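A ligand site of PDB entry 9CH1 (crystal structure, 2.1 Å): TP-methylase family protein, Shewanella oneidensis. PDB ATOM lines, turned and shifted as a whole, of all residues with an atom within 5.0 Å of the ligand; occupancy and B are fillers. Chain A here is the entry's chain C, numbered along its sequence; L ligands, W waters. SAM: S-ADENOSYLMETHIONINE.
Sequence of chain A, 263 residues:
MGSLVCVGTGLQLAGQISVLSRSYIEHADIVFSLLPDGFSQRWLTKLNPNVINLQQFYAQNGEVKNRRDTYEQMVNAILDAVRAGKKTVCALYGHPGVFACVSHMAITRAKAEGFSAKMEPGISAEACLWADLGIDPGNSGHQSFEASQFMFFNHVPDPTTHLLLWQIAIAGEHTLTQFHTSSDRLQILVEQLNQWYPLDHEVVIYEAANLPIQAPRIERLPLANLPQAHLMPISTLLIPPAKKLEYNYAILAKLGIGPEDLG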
ATOM      1  N   LEU A  11      19.248 -12.353  -1.382  1.00  0.00           N
ATOM      2  CA  LEU A  11      18.968 -11.403  -2.441  1.00  0.00           C
ATOM      3  C   LEU A  11      20.277 -10.859  -3.022  1.00  0.00           C
ATOM      4  O   LEU A  11      20.390 -10.710  -4.235  1.00  0.00           O
ATOM      5  CB  LEU A  11      18.068 -10.292  -1.910  1.00  0.00           C
ATOM      6  CG  LEU A  11      16.556 -10.591  -1.922  1.00  0.00           C
ATOM      7  CD1 LEU A  11      16.016 -10.565  -3.337  1.00  0.00           C
ATOM      8  CD2 LEU A  11      16.246 -11.925  -1.271  1.00  0.00           C
ATOM      9  N   TYR A  93      16.613 -18.026  -5.016  1.00  0.00           N
ATOM     10  CA  TYR A  93      17.013 -16.755  -4.446  1.00  0.00           C
ATOM     11  C   TYR A  93      16.131 -16.461  -3.225  1.00  0.00           C
ATOM     12  O   TYR A  93      14.975 -16.882  -3.163  1.00  0.00           O
ATOM     13  CB  TYR A  93      16.943 -15.628  -5.476  1.00  0.00           C
ATOM     14  CG  TYR A  93      15.548 -15.152  -5.845  1.00  0.00           C
ATOM     15  CD1 TYR A  93      14.894 -14.186  -5.099  1.00  0.00           C
ATOM     16  CD2 TYR A  93      14.885 -15.664  -6.962  1.00  0.00           C
ATOM     17  CE1 TYR A  93      13.623 -13.740  -5.426  1.00  0.00           C
ATOM     18  CE2 TYR A  93      13.610 -15.226  -7.300  1.00  0.00           C
ATOM     19  CZ  TYR A  93      12.977 -14.268  -6.537  1.00  0.00           C
ATOM     20  OH  TYR A  93      11.731 -13.839  -6.879  1.00  0.00           O
ATOM     21  N   GLY A  94      16.704 -15.728  -2.271  1.00  0.00           N
ATOM     22  CA  GLY A  94      16.030 -15.425  -1.012  1.00  0.00           C
ATOM     23  C   GLY A  94      15.908 -16.670  -0.127  1.00  0.00           C
ATOM     24  O   GLY A  94      16.879 -17.420   0.032  1.00  0.00           O
ATOM     25  N   HIS A  95      14.716 -16.858   0.437  1.00  0.00           N
ATOM     26  CA  HIS A  95      14.378 -18.030   1.225  1.00  0.00           C
ATOM     27  C   HIS A  95      13.588 -18.978   0.339  1.00  0.00           C
ATOM     28  O   HIS A  95      12.605 -18.576  -0.282  1.00  0.00           O
ATOM     29  CB  HIS A  95      13.640 -17.583   2.490  1.00  0.00           C
ATOM     30  CG  HIS A  95      13.220 -18.683   3.430  1.00  0.00           C
ATOM     31  ND1 HIS A  95      12.678 -19.876   3.020  1.00  0.00           N
ATOM     32  CD2 HIS A  95      13.241 -18.716   4.764  1.00  0.00           C
ATOM     33  CE1 HIS A  95      12.401 -20.613   4.093  1.00  0.00           C
ATOM     34  NE2 HIS A  95      12.737 -19.927   5.160  1.00  0.00           N
ATOM     35  N   VAL A  98       9.707 -19.144   0.913  1.00  0.00           N
ATOM     36  CA  VAL A  98       8.963 -17.914   1.156  1.00  0.00           C
ATOM     37  C   VAL A  98       8.390 -17.416  -0.172  1.00  0.00           C
ATOM     38  O   VAL A  98       9.139 -16.984  -1.047  1.00  0.00           O
ATOM     39  CB  VAL A  98       9.830 -16.844   1.846  1.00  0.00           C
ATOM     40  CG1 VAL A  98       9.161 -15.477   1.855  1.00  0.00           C
ATOM     41  CG2 VAL A  98      10.209 -17.263   3.269  1.00  0.00           C
ATOM     42  N   PHE A  99       7.064 -17.477  -0.285  1.00  0.00           N
ATOM     43  CA  PHE A  99       6.363 -17.151  -1.519  1.00  0.00           C
ATOM     44  C   PHE A  99       7.024 -17.900  -2.674  1.00  0.00           C
ATOM     45  O   PHE A  99       7.365 -17.302  -3.701  1.00  0.00           O
ATOM     46  CB  PHE A  99       6.340 -15.637  -1.731  1.00  0.00           C
ATOM     47  CG  PHE A  99       5.366 -14.898  -0.814  1.00  0.00           C
ATOM     48  CD1 PHE A  99       5.677 -14.637   0.504  1.00  0.00           C
ATOM     49  CD2 PHE A  99       4.127 -14.477  -1.301  1.00  0.00           C
ATOM     50  CE1 PHE A  99       4.795 -13.969   1.329  1.00  0.00           C
ATOM     51  CE2 PHE A  99       3.239 -13.797  -0.464  1.00  0.00           C
ATOM     52  CZ  PHE A  99       3.575 -13.554   0.849  1.00  0.00           C
ATOM     53  N   ALA A 100       7.192 -19.212  -2.494  1.00  0.00           N
ATOM     54  CA  ALA A 100       7.792 -20.073  -3.503  1.00  0.00           C
ATOM     55  C   ALA A 100       7.290 -21.505  -3.310  1.00  0.00           C
ATOM     56  O   ALA A 100       7.583 -22.150  -2.303  1.00  0.00           O
ATOM     57  CB  ALA A 100       9.306 -20.002  -3.411  1.00  0.00           C
ATOM     58  N   ILE A 123      17.610 -15.953   3.575  1.00  0.00           N
ATOM     59  CA  ILE A 123      17.270 -14.572   3.851  1.00  0.00           C
ATOM     60  C   ILE A 123      16.336 -14.065   2.750  1.00  0.00           C
ATOM     61  O   ILE A 123      16.718 -14.030   1.582  1.00  0.00           O
ATOM     62  CB  ILE A 123      18.549 -13.717   4.005  1.00  0.00           C
ATOM     63  CG1 ILE A 123      19.342 -14.134   5.247  1.00  0.00           C
ATOM     64  CG2 ILE A 123      18.219 -12.229   4.020  1.00  0.00           C
ATOM     65  CD1 ILE A 123      20.778 -13.655   5.261  1.00  0.00           C
ATOM     66  N   SER A 124      15.121 -13.675   3.151  1.00  0.00           N
ATOM     67  CA  SER A 124      14.064 -13.326   2.217  1.00  0.00           C
ATOM     68  C   SER A 124      13.996 -11.820   1.999  1.00  0.00           C
ATOM     69  O   SER A 124      14.656 -11.045   2.695  1.00  0.00           O
ATOM     70  CB  SER A 124      12.734 -13.853   2.701  1.00  0.00           C
ATOM     71  OG  SER A 124      12.284 -13.134   3.847  1.00  0.00           O
ATOM     72  N   ALA A 125      13.171 -11.409   1.025  1.00  0.00           N
ATOM     73  CA  ALA A 125      12.976 -10.001   0.709  1.00  0.00           C
ATOM     74  C   ALA A 125      12.402  -9.273   1.921  1.00  0.00           C
ATOM     75  O   ALA A 125      12.702  -8.096   2.154  1.00  0.00           O
ATOM     76  CB  ALA A 125      12.068  -9.868  -0.496  1.00  0.00           C
ATOM     77  N   GLU A 126      11.568  -9.983   2.678  1.00  0.00           N
ATOM     78  CA  GLU A 126      10.992  -9.465   3.913  1.00  0.00           C
ATOM     79  C   GLU A 126      12.120  -9.128   4.890  1.00  0.00           C
ATOM     80  O   GLU A 126      12.142  -8.063   5.487  1.00  0.00           O
ATOM     81  CB  GLU A 126      10.050 -10.550   4.439  1.00  0.00           C
ATOM     82  CG  GLU A 126       9.235 -10.128   5.660  1.00  0.00           C
ATOM     83  CD  GLU A 126       8.139 -11.127   5.992  1.00  0.00           C
ATOM     84  OE1 GLU A 126       7.131 -11.168   5.254  1.00  0.00           O
ATOM     85  OE2 GLU A 126       8.296 -11.878   6.981  1.00  0.00           O
ATOM     86  N   LEU A 165       2.307  -6.322   0.586  1.00  0.00           N
ATOM     87  CA  LEU A 165       1.691  -7.005  -0.529  1.00  0.00           C
ATOM     88  C   LEU A 165       2.784  -7.428  -1.508  1.00  0.00           C
ATOM     89  O   LEU A 165       3.423  -6.590  -2.133  1.00  0.00           O
ATOM     90  CB  LEU A 165       0.656  -6.112  -1.210  1.00  0.00           C
ATOM     91  CG  LEU A 165      -0.518  -5.656  -0.338  1.00  0.00           C
ATOM     92  CD1 LEU A 165      -1.581  -4.988  -1.199  1.00  0.00           C
ATOM     93  CD2 LEU A 165      -1.107  -6.816   0.441  1.00  0.00           C
ATOM     94  N   TRP A 166       3.001  -8.748  -1.609  1.00  0.00           N
ATOM     95  CA  TRP A 166       4.021  -9.305  -2.486  1.00  0.00           C
ATOM     96  C   TRP A 166       3.460  -9.430  -3.899  1.00  0.00           C
ATOM     97  O   TRP A 166       2.247  -9.495  -4.098  1.00  0.00           O
ATOM     98  CB  TRP A 166       4.489 -10.676  -1.964  1.00  0.00           C
ATOM     99  CG  TRP A 166       5.077 -10.661  -0.579  1.00  0.00           C
ATOM    100  CD1 TRP A 166       4.524 -10.162   0.570  1.00  0.00           C
ATOM    101  CD2 TRP A 166       6.380 -11.174  -0.194  1.00  0.00           C
ATOM    102  NE1 TRP A 166       5.374 -10.348   1.632  1.00  0.00           N
ATOM    103  CE2 TRP A 166       6.522 -10.954   1.190  1.00  0.00           C
ATOM    104  CE3 TRP A 166       7.421 -11.797  -0.889  1.00  0.00           C
ATOM    105  CZ2 TRP A 166       7.670 -11.339   1.896  1.00  0.00           C
ATOM    106  CZ3 TRP A 166       8.549 -12.175  -0.191  1.00  0.00           C
ATOM    107  CH2 TRP A 166       8.669 -11.948   1.177  1.00  0.00           C
ATOM    108  N   GLN A 167       4.360  -9.449  -4.893  1.00  0.00           N
ATOM    109  CA  GLN A 167       3.993  -9.644  -6.287  1.00  0.00           C
ATOM    110  C   GLN A 167       2.966  -8.600  -6.716  1.00  0.00           C
ATOM    111  O   GLN A 167       1.976  -8.925  -7.372  1.00  0.00           O
ATOM    112  CB  GLN A 167       3.470 -11.059  -6.516  1.00  0.00           C
ATOM    113  CG  GLN A 167       4.345 -12.150  -5.902  1.00  0.00           C
ATOM    114  CD  GLN A 167       4.064 -13.530  -6.460  1.00  0.00           C
ATOM    115  OE1 GLN A 167       2.915 -13.928  -6.660  1.00  0.00           O
ATOM    116  NE2 GLN A 167       5.138 -14.267  -6.738  1.00  0.00           N
ATOM    117  N   ILE A 168       3.225  -7.340  -6.355  1.00  0.00           N
ATOM    118  CA  ILE A 168       2.284  -6.245  -6.594  1.00  0.00           C
ATOM    119  C   ILE A 168       2.211  -5.960  -8.101  1.00  0.00           C
ATOM    120  O   ILE A 168       1.227  -5.385  -8.567  1.00  0.00           O
ATOM    121  CB  ILE A 168       2.683  -4.998  -5.784  1.00  0.00           C
ATOM    122  CG1 ILE A 168       1.673  -3.860  -5.938  1.00  0.00           C
ATOM    123  CG2 ILE A 168       4.097  -4.539  -6.145  1.00  0.00           C
ATOM    124  CD1 ILE A 168       0.319  -4.144  -5.306  1.00  0.00           C
ATOM    125  N   TYR A 206       9.255  -1.073  -2.468  1.00  0.00           N
ATOM    126  CA  TYR A 206      10.571  -1.504  -2.013  1.00  0.00           C
ATOM    127  C   TYR A 206      11.126  -2.568  -2.953  1.00  0.00           C
ATOM    128  O   TYR A 206      10.409  -3.466  -3.394  1.00  0.00           O
ATOM    129  CB  TYR A 206      10.489  -2.040  -0.581  1.00  0.00           C
ATOM    130  CG  TYR A 206      11.758  -2.730  -0.104  1.00  0.00           C
ATOM    131  CD1 TYR A 206      12.900  -1.995   0.193  1.00  0.00           C
ATOM    132  CD2 TYR A 206      11.817  -4.112   0.040  1.00  0.00           C
ATOM    133  CE1 TYR A 206      14.064  -2.619   0.621  1.00  0.00           C
ATOM    134  CE2 TYR A 206      12.978  -4.745   0.466  1.00  0.00           C
ATOM    135  CZ  TYR A 206      14.103  -3.994   0.757  1.00  0.00           C
ATOM    136  OH  TYR A 206      15.250  -4.601   1.179  1.00  0.00           O
ATOM    137  N   GLU A 207      12.427  -2.437  -3.254  1.00  0.00           N
ATOM    138  CA  GLU A 207      13.176  -3.454  -3.977  1.00  0.00           C
ATOM    139  C   GLU A 207      14.551  -3.585  -3.336  1.00  0.00           C
ATOM    140  O   GLU A 207      15.367  -2.674  -3.423  1.00  0.00           O
ATOM    141  CB  GLU A 207      13.323  -3.110  -5.452  1.00  0.00           C
ATOM    142  CG  GLU A 207      11.989  -2.930  -6.183  1.00  0.00           C
ATOM    143  CD  GLU A 207      12.128  -2.484  -7.623  1.00  0.00           C
ATOM    144  OE1 GLU A 207      13.276  -2.354  -8.099  1.00  0.00           O
ATOM    145  OE2 GLU A 207      11.084  -2.250  -8.270  1.00  0.00           O
ATOM    146  N   ALA A 208      14.804  -4.737  -2.697  1.00  0.00           N
ATOM    147  CA  ALA A 208      16.118  -5.057  -2.186  1.00  0.00           C
ATOM    148  C   ALA A 208      17.105  -5.158  -3.344  1.00  0.00           C
ATOM    149  O   ALA A 208      16.755  -5.618  -4.430  1.00  0.00           O
ATOM    150  CB  ALA A 208      16.061  -6.353  -1.397  1.00  0.00           C
ATOM    151  N   ASN A 210      20.261  -6.534  -5.551  1.00  0.00           N
ATOM    152  CA  ASN A 210      20.777  -7.856  -5.881  1.00  0.00           C
ATOM    153  C   ASN A 210      22.297  -7.802  -6.055  1.00  0.00           C
ATOM    154  O   ASN A 210      22.953  -8.841  -6.059  1.00  0.00           O
ATOM    155  CB  ASN A 210      20.110  -8.428  -7.117  1.00  0.00           C
ATOM    156  CG  ASN A 210      18.631  -8.697  -6.905  1.00  0.00           C
ATOM    157  OD1 ASN A 210      18.272  -9.523  -6.058  1.00  0.00           O
ATOM    158  ND2 ASN A 210      17.778  -8.017  -7.657  1.00  0.00           N
ATOM    159  N   PRO A 233       8.794  -7.024 -11.428  1.00  0.00           N
ATOM    160  CA  PRO A 233       8.477  -8.321 -10.822  1.00  0.00           C
ATOM    161  C   PRO A 233       9.017  -8.462  -9.402  1.00  0.00           C
ATOM    162  O   PRO A 233       8.465  -9.207  -8.592  1.00  0.00           O
ATOM    163  CB  PRO A 233       9.116  -9.334 -11.786  1.00  0.00           C
ATOM    164  CG  PRO A 233       9.184  -8.605 -13.109  1.00  0.00           C
ATOM    165  CD  PRO A 233       9.447  -7.150 -12.732  1.00  0.00           C
ATOM    166  N   ILE A 234      10.103  -7.742  -9.100  1.00  0.00           N
ATOM    167  CA  ILE A 234      10.793  -7.902  -7.832  1.00  0.00           C
ATOM    168  C   ILE A 234      10.255  -6.904  -6.802  1.00  0.00           C
ATOM    169  O   ILE A 234      10.723  -6.881  -5.666  1.00  0.00           O
ATOM    170  CB  ILE A 234      12.318  -7.755  -8.005  1.00  0.00           C
ATOM    171  CG1 ILE A 234      12.718  -6.368  -8.508  1.00  0.00           C
ATOM    172  CG2 ILE A 234      12.879  -8.857  -8.900  1.00  0.00           C
ATOM    173  CD1 ILE A 234      14.172  -6.021  -8.280  1.00  0.00           C
ATOM    174  N   SER A 235       9.262  -6.092  -7.204  1.00  0.00           N
ATOM    175  CA  SER A 235       8.743  -5.053  -6.333  1.00  0.00           C
ATOM    176  C   SER A 235       7.844  -5.651  -5.249  1.00  0.00           C
ATOM    177  O   SER A 235       7.043  -6.530  -5.524  1.00  0.00           O
ATOM    178  CB  SER A 235       8.010  -3.997  -7.120  1.00  0.00           C
ATOM    179  OG  SER A 235       8.867  -3.312  -8.015  1.00  0.00           O
ATOM    180  N   THR A 236       7.998  -5.147  -4.021  1.00  0.00           N
ATOM    181  CA  THR A 236       7.070  -5.432  -2.942  1.00  0.00           C
ATOM    182  C   THR A 236       6.512  -4.107  -2.414  1.00  0.00           C
ATOM    183  O   THR A 236       7.242  -3.128  -2.299  1.00  0.00           O
ATOM    184  CB  THR A 236       7.793  -6.214  -1.833  1.00  0.00           C
ATOM    185  OG1 THR A 236       8.118  -7.489  -2.388  1.00  0.00           O
ATOM    186  CG2 THR A 236       6.922  -6.414  -0.608  1.00  0.00           C
HETATM  187  N   SAM L   1      11.643 -16.467  -2.252  1.00  0.00           N
HETATM  188  CA  SAM L   1      11.663 -15.004  -2.506  1.00  0.00           C
HETATM  189  C   SAM L   1      12.055 -14.284  -1.207  1.00  0.00           C
HETATM  190  O   SAM L   1      12.602 -14.972  -0.318  1.00  0.00           O
HETATM  191  OXT SAM L   1      11.810 -13.059  -1.125  1.00  0.00           O
HETATM  192  CB  SAM L   1      10.304 -14.516  -2.999  1.00  0.00           C
HETATM  193  CG  SAM L   1       9.985 -14.929  -4.439  1.00  0.00           C
HETATM  194  SD  SAM L   1       8.276 -14.551  -4.895  1.00  0.00           S
HETATM  195  CE  SAM L   1       7.955 -15.732  -6.193  1.00  0.00           C
HETATM  196  C5' SAM L   1       8.555 -13.024  -5.822  1.00  0.00           C
HETATM  197  C4' SAM L   1       8.145 -11.823  -5.002  1.00  0.00           C
HETATM  198  O4' SAM L   1       9.063 -11.667  -3.903  1.00  0.00           O
HETATM  199  C3' SAM L   1       8.154 -10.478  -5.718  1.00  0.00           C
HETATM  200  O3' SAM L   1       6.943 -10.272  -6.440  1.00  0.00           O
HETATM  201  C2' SAM L   1       8.300  -9.529  -4.521  1.00  0.00           C
HETATM  202  O2' SAM L   1       7.086  -9.349  -3.813  1.00  0.00           O
HETATM  203  C1' SAM L   1       9.311 -10.296  -3.678  1.00  0.00           C
HETATM  204  N9  SAM L   1      10.692  -9.983  -4.055  1.00  0.00           N
HETATM  205  C8  SAM L   1      11.537 -10.740  -4.826  1.00  0.00           C
HETATM  206  N7  SAM L   1      12.705 -10.175  -5.002  1.00  0.00           N
HETATM  207  C5  SAM L   1      12.623  -8.974  -4.303  1.00  0.00           C
HETATM  208  C6  SAM L   1      13.542  -7.923  -4.110  1.00  0.00           C
HETATM  209  N6  SAM L   1      14.770  -7.908  -4.611  1.00  0.00           N
HETATM  210  N1  SAM L   1      13.132  -6.872  -3.362  1.00  0.00           N
HETATM  211  C2  SAM L   1      11.883  -6.891  -2.860  1.00  0.00           C
HETATM  212  N3  SAM L   1      10.947  -7.820  -2.973  1.00  0.00           N
HETATM  213  C4  SAM L   1      11.385  -8.847  -3.722  1.00  0.00           C
HETATM  214  O   HOH W   1       5.873  -7.293  -7.894  1.00  0.00           O
HETATM  215  O   HOH W   2      15.309 -10.331  -6.259  1.00  0.00           O
HETATM  216  O   HOH W   3      12.683 -17.677  -4.530  1.00  0.00           O
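The backbone carbonyl oxygen (O) of Phe 99 sits close to a sulfur (SD) of the ligand.
The backbone carbonyl oxygen (O) of Ile 234 lies close to a nitrogen (N3) of the ligand.
Merely in contact with the ligand: Leu 11 (3.2 Å), Gly 94 (3.5 Å), Ser 124 (3.2 Å), Trp 166 (3.3 Å), Tyr 206 (3.8 Å) and Glu 207 (3.5 Å).
Hydrophobic or aromatic side chains that line the ligand: Leu 11, Tyr 93, His 95, Val 98, Phe 99, Ala 125, Trp 166, Ala 208 and Ile 234.
O of Thr 236 is in hydrogen-bond range of N of Tyr 206.
The backbone carbonyl oxygen of Leu 11 lies close to the side-chain amide oxygen of Asn 210 (3.0 Å).
N of Glu 126 sits close to OG of Ser 124 (3.4 Å).
OG of Ser 235 lies within hydrogen-bond range of OE2 of Glu 207.
An oxygen (O2') of the ligand sits at hydrogen-bond distance from the side-chain hydroxyl of Thr 236.
The backbone NH (N) of Ala 208 is in hydrogen-bond range of a nitrogen (N1) of the ligand (2.8 Å).
The backbone carbonyl oxygen of Ala 208 is in hydrogen-bond range of a nitrogen (N6) of the ligand (3.0 Å).
O of Val 98 lies within hydrogen-bond range of N of the ligand, 2.8 Å away.
O3' of the ligand is in hydrogen-bond range of O of Pro 233 (2.8 Å).
N of His 95 sits at hydrogen-bond distance from O of the ligand (2.9 Å).
The backbone carbonyl oxygen (O) of His 95 lies within hydrogen-bond range of a nitrogen (N) of the ligand.
The backbone NH (N) of Gln 167 is in hydrogen-bond range of an oxygen (O2') of the ligand.
N of Ala 125 is in hydrogen-bond range of OXT of the ligand (3.0 Å).
The backbone carbonyl oxygen of Tyr 93 lies within hydrogen-bond range of a nitrogen (N) of the ligand (3.5 Å).
An oxygen (O2') of the ligand sits at hydrogen-bond distance from the backbone carbonyl oxygen (O) of Ser 235, 3.3 Å away.
Water W3 bridges a nitrogen (N) of the ligand (2.8 Å) and the backbone carbonyl oxygen of Tyr 93 (2.8 Å).
Water W2 lies within hydrogen-bond range of N7 of the ligand (2.9 Å) and OD1 of Asn 210 (3.1 Å).
Water W1 lies within hydrogen-bond range of the backbone carbonyl oxygen (O) of Ser 235 (2.8 Å), the backbone NH (N) of Ile 168 (3.1 Å), the backbone carbonyl oxygen (O) of Pro 233 (3.3 Å) and an oxygen (O3') of the ligand (3.5 Å).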
